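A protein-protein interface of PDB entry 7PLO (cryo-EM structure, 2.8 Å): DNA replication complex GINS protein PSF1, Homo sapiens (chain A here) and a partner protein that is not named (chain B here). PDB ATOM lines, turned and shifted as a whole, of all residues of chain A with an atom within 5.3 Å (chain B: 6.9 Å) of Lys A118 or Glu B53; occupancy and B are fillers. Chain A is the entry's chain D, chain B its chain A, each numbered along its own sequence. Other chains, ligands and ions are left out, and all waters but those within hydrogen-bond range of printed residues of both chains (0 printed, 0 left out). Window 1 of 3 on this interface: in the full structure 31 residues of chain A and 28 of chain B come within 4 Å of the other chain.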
ATOM      1  N   ARG A  91     -28.815   5.227  27.161  1.00  0.00           N
ATOM      2  CA  ARG A  91     -27.522   5.862  26.893  1.00  0.00           C
ATOM      3  C   ARG A  91     -26.632   4.960  26.052  1.00  0.00           C
ATOM      4  O   ARG A  91     -25.936   5.430  25.144  1.00  0.00           O
ATOM      5  CB  ARG A  91     -26.825   6.216  28.214  1.00  0.00           C
ATOM      6  CG  ARG A  91     -25.367   6.726  28.108  1.00  0.00           C
ATOM      7  CD  ARG A  91     -25.232   7.973  27.241  1.00  0.00           C
ATOM      8  NE  ARG A  91     -23.846   8.431  27.141  1.00  0.00           N
ATOM      9  CZ  ARG A  91     -22.975   8.081  26.201  1.00  0.00           C
ATOM     10  NH1 ARG A  91     -23.291   7.246  25.222  1.00  0.00           N
ATOM     11  NH2 ARG A  91     -21.744   8.584  26.242  1.00  0.00           N
ATOM     12  N   SER A  96     -26.466  10.065  23.615  1.00  0.00           N
ATOM     13  CA  SER A  96     -26.591  11.066  24.669  1.00  0.00           C
ATOM     14  C   SER A  96     -27.841  11.928  24.514  1.00  0.00           C
ATOM     15  O   SER A  96     -28.575  12.133  25.485  1.00  0.00           O
ATOM     16  CB  SER A  96     -25.344  11.953  24.689  1.00  0.00           C
ATOM     17  OG  SER A  96     -25.419  12.925  25.716  1.00  0.00           O
ATOM     18  N   VAL A  97     -28.088  12.446  23.312  1.00  0.00           N
ATOM     19  CA  VAL A  97     -29.244  13.299  23.045  1.00  0.00           C
ATOM     20  C   VAL A  97     -30.373  12.379  22.593  1.00  0.00           C
ATOM     21  O   VAL A  97     -30.399  11.923  21.450  1.00  0.00           O
ATOM     22  CB  VAL A  97     -28.928  14.378  22.004  1.00  0.00           C
ATOM     23  CG1 VAL A  97     -30.169  15.231  21.689  1.00  0.00           C
ATOM     24  CG2 VAL A  97     -27.775  15.269  22.486  1.00  0.00           C
ATOM     25  N   MET A 111     -35.115  13.189  33.675  1.00  0.00           N
ATOM     26  CA  MET A 111     -34.104  13.831  32.843  1.00  0.00           C
ATOM     27  C   MET A 111     -32.933  14.320  33.686  1.00  0.00           C
ATOM     28  O   MET A 111     -31.779  14.254  33.250  1.00  0.00           O
ATOM     29  CB  MET A 111     -34.723  14.987  32.057  1.00  0.00           C
ATOM     30  CG  MET A 111     -33.855  15.513  30.914  1.00  0.00           C
ATOM     31  SD  MET A 111     -33.675  14.345  29.550  1.00  0.00           S
ATOM     32  CE  MET A 111     -32.528  15.226  28.493  1.00  0.00           C
ATOM     33  N   TRP A 113     -31.884  12.912  36.519  1.00  0.00           N
ATOM     34  CA  TRP A 113     -31.131  11.702  36.838  1.00  0.00           C
ATOM     35  C   TRP A 113     -30.305  11.250  35.644  1.00  0.00           C
ATOM     36  O   TRP A 113     -29.150  10.841  35.797  1.00  0.00           O
ATOM     37  CB  TRP A 113     -32.081  10.582  37.273  1.00  0.00           C
ATOM     38  CG  TRP A 113     -31.378   9.316  37.714  1.00  0.00           C
ATOM     39  CD1 TRP A 113     -31.061   8.963  38.992  1.00  0.00           C
ATOM     40  CD2 TRP A 113     -30.911   8.244  36.877  1.00  0.00           C
ATOM     41  NE1 TRP A 113     -30.425   7.746  39.004  1.00  0.00           N
ATOM     42  CE2 TRP A 113     -30.321   7.285  37.719  1.00  0.00           C
ATOM     43  CE3 TRP A 113     -30.938   8.005  35.499  1.00  0.00           C
ATOM     44  CZ2 TRP A 113     -29.763   6.107  37.230  1.00  0.00           C
ATOM     45  CZ3 TRP A 113     -30.380   6.839  35.017  1.00  0.00           C
ATOM     46  CH2 TRP A 113     -29.802   5.903  35.880  1.00  0.00           C
ATOM     47  N   PHE A 114     -30.892  11.296  34.448  1.00  0.00           N
ATOM     48  CA  PHE A 114     -30.184  10.860  33.253  1.00  0.00           C
ATOM     49  C   PHE A 114     -28.997  11.767  32.954  1.00  0.00           C
ATOM     50  O   PHE A 114     -27.936  11.289  32.546  1.00  0.00           O
ATOM     51  CB  PHE A 114     -31.154  10.815  32.074  1.00  0.00           C
ATOM     52  CG  PHE A 114     -30.563  10.251  30.814  1.00  0.00           C
ATOM     53  CD1 PHE A 114     -30.085   8.953  30.773  1.00  0.00           C
ATOM     54  CD2 PHE A 114     -30.512  11.012  29.662  1.00  0.00           C
ATOM     55  CE1 PHE A 114     -29.552   8.435  29.616  1.00  0.00           C
ATOM     56  CE2 PHE A 114     -29.979  10.497  28.500  1.00  0.00           C
ATOM     57  CZ  PHE A 114     -29.500   9.207  28.477  1.00  0.00           C
ATOM     58  N   ASN A 115     -29.156  13.078  33.152  1.00  0.00           N
ATOM     59  CA  ASN A 115     -28.039  13.996  32.955  1.00  0.00           C
ATOM     60  C   ASN A 115     -26.926  13.736  33.962  1.00  0.00           C
ATOM     61  O   ASN A 115     -25.740  13.755  33.604  1.00  0.00           O
ATOM     62  CB  ASN A 115     -28.524  15.440  33.053  1.00  0.00           C
ATOM     63  CG  ASN A 115     -29.443  15.827  31.911  1.00  0.00           C
ATOM     64  OD1 ASN A 115     -29.446  15.192  30.858  1.00  0.00           O
ATOM     65  ND2 ASN A 115     -30.224  16.880  32.113  1.00  0.00           N
ATOM     66  N   ASN A 116     -27.284  13.490  35.227  1.00  0.00           N
ATOM     67  CA  ASN A 116     -26.270  13.146  36.221  1.00  0.00           C
ATOM     68  C   ASN A 116     -25.555  11.853  35.852  1.00  0.00           C
ATOM     69  O   ASN A 116     -24.330  11.748  35.996  1.00  0.00           O
ATOM     70  CB  ASN A 116     -26.904  13.022  37.607  1.00  0.00           C
ATOM     71  CG  ASN A 116     -27.287  14.360  38.205  1.00  0.00           C
ATOM     72  OD1 ASN A 116     -26.786  15.408  37.798  1.00  0.00           O
ATOM     73  ND2 ASN A 116     -28.175  14.330  39.191  1.00  0.00           N
ATOM     74  N   TYR A 117     -26.304  10.856  35.376  1.00  0.00           N
ATOM     75  CA  TYR A 117     -25.694   9.590  34.982  1.00  0.00           C
ATOM     76  C   TYR A 117     -24.758   9.774  33.795  1.00  0.00           C
ATOM     77  O   TYR A 117     -23.672   9.187  33.760  1.00  0.00           O
ATOM     78  CB  TYR A 117     -26.774   8.562  34.651  1.00  0.00           C
ATOM     79  CG  TYR A 117     -26.213   7.288  34.065  1.00  0.00           C
ATOM     80  CD1 TYR A 117     -25.529   6.382  34.862  1.00  0.00           C
ATOM     81  CD2 TYR A 117     -26.357   6.996  32.717  1.00  0.00           C
ATOM     82  CE1 TYR A 117     -25.008   5.222  34.334  1.00  0.00           C
ATOM     83  CE2 TYR A 117     -25.838   5.836  32.181  1.00  0.00           C
ATOM     84  CZ  TYR A 117     -25.164   4.954  32.993  1.00  0.00           C
ATOM     85  OH  TYR A 117     -24.647   3.795  32.466  1.00  0.00           O
ATOM     86  N   LYS A 118     -25.170  10.573  32.807  1.00  0.00           N
ATOM     87  CA  LYS A 118     -24.308  10.856  31.664  1.00  0.00           C
ATOM     88  C   LYS A 118     -23.023  11.541  32.103  1.00  0.00           C
ATOM     89  O   LYS A 118     -21.931  11.181  31.649  1.00  0.00           O
ATOM     90  CB  LYS A 118     -25.042  11.738  30.655  1.00  0.00           C
ATOM     91  CG  LYS A 118     -26.090  11.031  29.808  1.00  0.00           C
ATOM     92  CD  LYS A 118     -26.586  11.916  28.661  1.00  0.00           C
ATOM     93  CE  LYS A 118     -27.424  13.099  29.143  1.00  0.00           C
ATOM     94  NZ  LYS A 118     -27.811  14.005  28.027  1.00  0.00           N
ATOM     95  N   ARG A 119     -23.138  12.530  32.993  1.00  0.00           N
ATOM     96  CA  ARG A 119     -21.959  13.248  33.467  1.00  0.00           C
ATOM     97  C   ARG A 119     -21.018  12.318  34.228  1.00  0.00           C
ATOM     98  O   ARG A 119     -19.797  12.349  34.021  1.00  0.00           O
ATOM     99  CB  ARG A 119     -22.400  14.424  34.340  1.00  0.00           C
ATOM    100  CG  ARG A 119     -21.438  15.602  34.354  1.00  0.00           C
ATOM    101  CD  ARG A 119     -21.981  16.797  35.146  1.00  0.00           C
ATOM    102  NE  ARG A 119     -23.241  17.313  34.607  1.00  0.00           N
ATOM    103  CZ  ARG A 119     -24.452  17.181  35.146  1.00  0.00           C
ATOM    104  NH1 ARG A 119     -24.651  16.567  36.303  1.00  0.00           N
ATOM    105  NH2 ARG A 119     -25.500  17.690  34.504  1.00  0.00           N
ATOM    106  N   SER A 120     -21.571  11.462  35.091  1.00  0.00           N
ATOM    107  CA  SER A 120     -20.741  10.536  35.858  1.00  0.00           C
ATOM    108  C   SER A 120     -20.072   9.503  34.958  1.00  0.00           C
ATOM    109  O   SER A 120     -18.897   9.164  35.155  1.00  0.00           O
ATOM    110  CB  SER A 120     -21.590   9.847  36.924  1.00  0.00           C
ATOM    111  OG  SER A 120     -20.804   8.975  37.714  1.00  0.00           O
ATOM    112  N   LEU A 121     -20.806   8.983  33.971  1.00  0.00           N
ATOM    113  CA  LEU A 121     -20.225   8.018  33.044  1.00  0.00           C
ATOM    114  C   LEU A 121     -19.118   8.655  32.217  1.00  0.00           C
ATOM    115  O   LEU A 121     -18.084   8.026  31.959  1.00  0.00           O
ATOM    116  CB  LEU A 121     -21.320   7.448  32.140  1.00  0.00           C
ATOM    117  CG  LEU A 121     -20.933   6.390  31.103  1.00  0.00           C
ATOM    118  CD1 LEU A 121     -20.362   5.146  31.762  1.00  0.00           C
ATOM    119  CD2 LEU A 121     -22.140   6.034  30.254  1.00  0.00           C
ATOM    120  N   ALA A 122     -19.319   9.904  31.786  1.00  0.00           N
ATOM    121  CA  ALA A 122     -18.272  10.610  31.057  1.00  0.00           C
ATOM    122  C   ALA A 122     -17.039  10.809  31.926  1.00  0.00           C
ATOM    123  O   ALA A 122     -15.909  10.672  31.447  1.00  0.00           O
ATOM    124  CB  ALA A 122     -18.800  11.951  30.553  1.00  0.00           C
ATOM    125  N   THR A 123     -17.239  11.125  33.210  1.00  0.00           N
ATOM    126  CA  THR A 123     -16.113  11.248  34.134  1.00  0.00           C
ATOM    127  C   THR A 123     -15.344   9.934  34.245  1.00  0.00           C
ATOM    128  O   THR A 123     -14.105   9.912  34.176  1.00  0.00           O
ATOM    129  CB  THR A 123     -16.627  11.689  35.509  1.00  0.00           C
ATOM    130  OG1 THR A 123     -17.300  12.948  35.390  1.00  0.00           O
ATOM    131  CG2 THR A 123     -15.491  11.823  36.522  1.00  0.00           C
ATOM    132  N   LEU B  16     -16.598  11.710  24.627  1.00  0.00           N
ATOM    133  CA  LEU B  16     -16.894  10.995  25.864  1.00  0.00           C
ATOM    134  C   LEU B  16     -18.234  11.429  26.428  1.00  0.00           C
ATOM    135  O   LEU B  16     -18.982  10.610  26.973  1.00  0.00           O
ATOM    136  CB  LEU B  16     -15.794  11.222  26.900  1.00  0.00           C
ATOM    137  CG  LEU B  16     -14.409  10.613  26.678  1.00  0.00           C
ATOM    138  CD1 LEU B  16     -13.552  10.911  27.887  1.00  0.00           C
ATOM    139  CD2 LEU B  16     -14.462   9.115  26.423  1.00  0.00           C
ATOM    140  N   ARG B  17     -18.561  12.716  26.301  1.00  0.00           N
ATOM    141  CA  ARG B  17     -19.886  13.182  26.688  1.00  0.00           C
ATOM    142  C   ARG B  17     -20.974  12.759  25.705  1.00  0.00           C
ATOM    143  O   ARG B  17     -22.154  13.008  25.974  1.00  0.00           O
ATOM    144  CB  ARG B  17     -19.842  14.698  26.856  1.00  0.00           C
ATOM    145  CG  ARG B  17     -19.048  15.115  28.108  1.00  0.00           C
ATOM    146  CD  ARG B  17     -19.900  15.744  29.212  1.00  0.00           C
ATOM    147  NE  ARG B  17     -21.176  15.061  29.417  1.00  0.00           N
ATOM    148  CZ  ARG B  17     -22.294  15.628  29.859  1.00  0.00           C
ATOM    149  NH1 ARG B  17     -22.341  16.900  30.229  1.00  0.00           N
ATOM    150  NH2 ARG B  17     -23.404  14.899  29.923  1.00  0.00           N
ATOM    151  N   LEU B  19     -21.213  13.325  22.122  1.00  0.00           N
ATOM    152  CA  LEU B  19     -21.612  14.379  21.203  1.00  0.00           C
ATOM    153  C   LEU B  19     -20.604  14.492  20.070  1.00  0.00           C
ATOM    154  O   LEU B  19     -19.402  14.298  20.275  1.00  0.00           O
ATOM    155  CB  LEU B  19     -21.729  15.711  21.946  1.00  0.00           C
ATOM    156  CG  LEU B  19     -22.785  15.758  23.056  1.00  0.00           C
ATOM    157  CD1 LEU B  19     -22.523  16.901  24.024  1.00  0.00           C
ATOM    158  CD2 LEU B  19     -24.183  15.863  22.464  1.00  0.00           C
ATOM    159  N   ILE B  48     -17.953  24.281  29.039  1.00  0.00           N
ATOM    160  CA  ILE B  48     -18.535  24.529  27.721  1.00  0.00           C
ATOM    161  C   ILE B  48     -19.555  23.452  27.369  1.00  0.00           C
ATOM    162  O   ILE B  48     -20.615  23.745  26.810  1.00  0.00           O
ATOM    163  CB  ILE B  48     -17.422  24.627  26.657  1.00  0.00           C
ATOM    164  CG1 ILE B  48     -16.613  25.912  26.859  1.00  0.00           C
ATOM    165  CG2 ILE B  48     -18.011  24.587  25.234  1.00  0.00           C
ATOM    166  CD1 ILE B  48     -15.254  25.899  26.202  1.00  0.00           C
ATOM    167  N   ILE B  49     -19.239  22.187  27.656  1.00  0.00           N
ATOM    168  CA  ILE B  49     -20.124  21.102  27.240  1.00  0.00           C
ATOM    169  C   ILE B  49     -21.411  21.122  28.058  1.00  0.00           C
ATOM    170  O   ILE B  49     -22.493  20.828  27.534  1.00  0.00           O
ATOM    171  CB  ILE B  49     -19.406  19.740  27.326  1.00  0.00           C
ATOM    172  CG1 ILE B  49     -18.245  19.672  26.323  1.00  0.00           C
ATOM    173  CG2 ILE B  49     -20.382  18.603  27.002  1.00  0.00           C
ATOM    174  CD1 ILE B  49     -17.181  18.640  26.655  1.00  0.00           C
ATOM    175  N   ASN B  50     -21.324  21.450  29.352  1.00  0.00           N
ATOM    176  CA  ASN B  50     -22.545  21.627  30.134  1.00  0.00           C
ATOM    177  C   ASN B  50     -23.393  22.764  29.568  1.00  0.00           C
ATOM    178  O   ASN B  50     -24.623  22.636  29.437  1.00  0.00           O
ATOM    179  CB  ASN B  50     -22.201  21.888  31.601  1.00  0.00           C
ATOM    180  CG  ASN B  50     -21.906  20.612  32.368  1.00  0.00           C
ATOM    181  OD1 ASN B  50     -22.821  19.915  32.808  1.00  0.00           O
ATOM    182  ND2 ASN B  50     -20.625  20.302  32.539  1.00  0.00           N
ATOM    183  N   ALA B  51     -22.743  23.875  29.197  1.00  0.00           N
ATOM    184  CA  ALA B  51     -23.467  24.985  28.583  1.00  0.00           C
ATOM    185  C   ALA B  51     -24.137  24.561  27.279  1.00  0.00           C
ATOM    186  O   ALA B  51     -25.262  24.984  26.985  1.00  0.00           O
ATOM    187  CB  ALA B  51     -22.515  26.155  28.340  1.00  0.00           C
ATOM    188  N   VAL B  52     -23.459  23.728  26.485  1.00  0.00           N
ATOM    189  CA  VAL B  52     -24.054  23.204  25.255  1.00  0.00           C
ATOM    190  C   VAL B  52     -25.277  22.361  25.583  1.00  0.00           C
ATOM    191  O   VAL B  52     -26.328  22.479  24.942  1.00  0.00           O
ATOM    192  CB  VAL B  52     -23.017  22.390  24.454  1.00  0.00           C
ATOM    193  CG1 VAL B  52     -23.688  21.569  23.350  1.00  0.00           C
ATOM    194  CG2 VAL B  52     -21.969  23.293  23.845  1.00  0.00           C
ATOM    195  N   GLU B  53     -25.154  21.486  26.584  1.00  0.00           N
ATOM    196  CA  GLU B  53     -26.253  20.595  26.933  1.00  0.00           C
ATOM    197  C   GLU B  53     -27.468  21.341  27.466  1.00  0.00           C
ATOM    198  O   GLU B  53     -28.568  20.777  27.457  1.00  0.00           O
ATOM    199  CB  GLU B  53     -25.801  19.561  27.970  1.00  0.00           C
ATOM    200  CG  GLU B  53     -25.123  18.323  27.390  1.00  0.00           C
ATOM    201  CD  GLU B  53     -25.288  17.104  28.276  1.00  0.00           C
ATOM    202  OE1 GLU B  53     -24.909  17.170  29.464  1.00  0.00           O
ATOM    203  OE2 GLU B  53     -25.812  16.081  27.786  1.00  0.00           O
ATOM    204  N   LYS B  54     -27.297  22.577  27.949  1.00  0.00           N
ATOM    205  CA  LYS B  54     -28.473  23.339  28.378  1.00  0.00           C
ATOM    206  C   LYS B  54     -29.467  23.575  27.238  1.00  0.00           C
ATOM    207  O   LYS B  54     -30.678  23.629  27.483  1.00  0.00           O
ATOM    208  CB  LYS B  54     -28.067  24.688  28.981  1.00  0.00           C
ATOM    209  CG  LYS B  54     -27.144  24.642  30.206  1.00  0.00           C
ATOM    210  CD  LYS B  54     -27.566  23.649  31.299  1.00  0.00           C
ATOM    211  CE  LYS B  54     -28.956  23.936  31.853  1.00  0.00           C
ATOM    212  NZ  LYS B  54     -29.304  23.013  32.971  1.00  0.00           N
ATOM    213  N   GLN B  55     -28.995  23.713  25.997  1.00  0.00           N
ATOM    214  CA  GLN B  55     -29.893  24.020  24.887  1.00  0.00           C
ATOM    215  C   GLN B  55     -30.771  22.815  24.539  1.00  0.00           C
ATOM    216  O   GLN B  55     -30.455  21.682  24.908  1.00  0.00           O
ATOM    217  CB  GLN B  55     -29.101  24.440  23.649  1.00  0.00           C
ATOM    218  CG  GLN B  55     -28.573  25.867  23.671  1.00  0.00           C
ATOM    219  CD  GLN B  55     -27.265  25.995  24.419  1.00  0.00           C
ATOM    220  OE1 GLN B  55     -26.189  25.863  23.838  1.00  0.00           O
ATOM    221  NE2 GLN B  55     -27.348  26.257  25.717  1.00  0.00           N
ATOM    222  N   PRO B  56     -31.900  23.035  23.817  1.00  0.00           N
ATOM    223  CA  PRO B  56     -32.723  21.886  23.371  1.00  0.00           C
ATOM    224  C   PRO B  56     -32.205  21.255  22.080  1.00  0.00           C
ATOM    225  O   PRO B  56     -32.701  21.476  20.974  1.00  0.00           O
ATOM    226  CB  PRO B  56     -34.104  22.519  23.187  1.00  0.00           C
ATOM    227  CG  PRO B  56     -33.802  23.896  22.727  1.00  0.00           C
ATOM    228  CD  PRO B  56     -32.535  24.315  23.444  1.00  0.00           C
ATOM    229  N   LEU B  57     -31.162  20.441  22.220  1.00  0.00           N
ATOM    230  CA  LEU B  57     -30.549  19.802  21.063  1.00  0.00           C
ATOM    231  C   LEU B  57     -31.470  18.745  20.470  1.00  0.00           C
ATOM    232  O   LEU B  57     -32.069  17.941  21.192  1.00  0.00           O
ATOM    233  CB  LEU B  57     -29.214  19.168  21.452  1.00  0.00           C
ATOM    234  CG  LEU B  57     -27.980  20.071  21.367  1.00  0.00           C
ATOM    235  CD1 LEU B  57     -28.120  21.313  22.238  1.00  0.00           C
ATOM    236  CD2 LEU B  57     -26.738  19.286  21.757  1.00  0.00           C
ATOM    237  N   VAL B  66     -24.464  26.476  17.989  1.00  0.00           N
ATOM    238  CA  VAL B  66     -24.657  25.999  19.354  1.00  0.00           C
ATOM    239  C   VAL B  66     -23.383  26.192  20.171  1.00  0.00           C
ATOM    240  O   VAL B  66     -23.438  26.616  21.331  1.00  0.00           O
ATOM    241  CB  VAL B  66     -25.124  24.530  19.341  1.00  0.00           C
ATOM    242  CG1 VAL B  66     -25.254  23.968  20.769  1.00  0.00           C
ATOM    243  CG2 VAL B  66     -26.455  24.397  18.582  1.00  0.00           C
ATOM    244  N   ALA B  70     -22.950  28.617  23.350  1.00  0.00           N
ATOM    245  CA  ALA B  70     -22.443  28.104  24.618  1.00  0.00           C
ATOM    246  C   ALA B  70     -21.282  28.942  25.134  1.00  0.00           C
ATOM    247  O   ALA B  70     -21.202  29.232  26.333  1.00  0.00           O
ATOM    248  CB  ALA B  70     -22.017  26.653  24.455  1.00  0.00           C
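NH2 of Arg A91 touches O of Leu B16, 3.5 Å away. Ser A96 touches Glu B53 (OG to OE2, 3.8 Å). CD2 of Leu B19 touches CG2 of Val A97, 3.6 Å away. Val A97 touches Leu B57 (CG1 to O, 3.3 Å). Arg B17 touches Lys A118 (NH2 to CB, 3.6 Å). Arg A119 touches Arg B17. Leu B16 touches Ala A122 (O to CB, 3.8 Å).
The backbone carbonyl oxygen of Ser A96 is in hydrogen-bond range of the side-chain amino group of Lys A118 (3.2 Å). The side-chain amide oxygen (OD1) of Asn A115 sits close to the side-chain amino group (NZ) of Lys A118, at 3.5 Å. The guanidinium group (NH1) of Arg A119 lies within hydrogen-bond range of the side-chain amide oxygen (OD1) of Asn A116. The backbone carbonyl oxygen (O) of Arg A119 lies within hydrogen-bond range of the side-chain hydroxyl (OG1) of Thr A123, 2.9 Å away. OE1 of Glu B53 lies within salt-bridge range of NH1 of Arg B17.
The backbone carbonyl oxygen (O) of Arg B17 lies within hydrogen-bond range of the side-chain hydroxyl (OG) of Ser A96. NZ of Lys A118 lies within salt-bridge range of OE2 of Glu B53 (2.9 Å). NE of Arg A119 lies within hydrogen-bond range of OD1 of Asn B50, at 3.2 Å.
Lys A118 touches two residues of chain B. Glu B53 touches just these residues of chain A: Ser A96 (3.8 Å) and Lys A118 (2.9 Å). Printed residues of chain A within 4 Å of Arg B17: Ser A96 (3.3 Å), Lys A118 (3.6 Å) and Arg A119 (3.9 Å). Of the printed residues of chain B, Ser A96 touches Arg B17 and Glu B53. Of the printed residues of chain A, Asn B50 touches Arg A119 (3.2 Å). Leu A121 touches none of the printed residues of chain B. The nearest residue of chain A that does not touch Glu B53 is Asn A115 (4.8 Å).
Hydrophobic or aromatic side chains of chain B within 4 Å of the printed part of chain A: Leu B19. Along chain B the printed residues that touch a printed residue of chain A span positions 16 to 57. Of the 15 printed residues of chain A, 6 touch a printed residue of chain B. Hydrophobic or aromatic side chains of chain A within 4 Å of the printed part of chain B: Val A97 and Ala A122.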
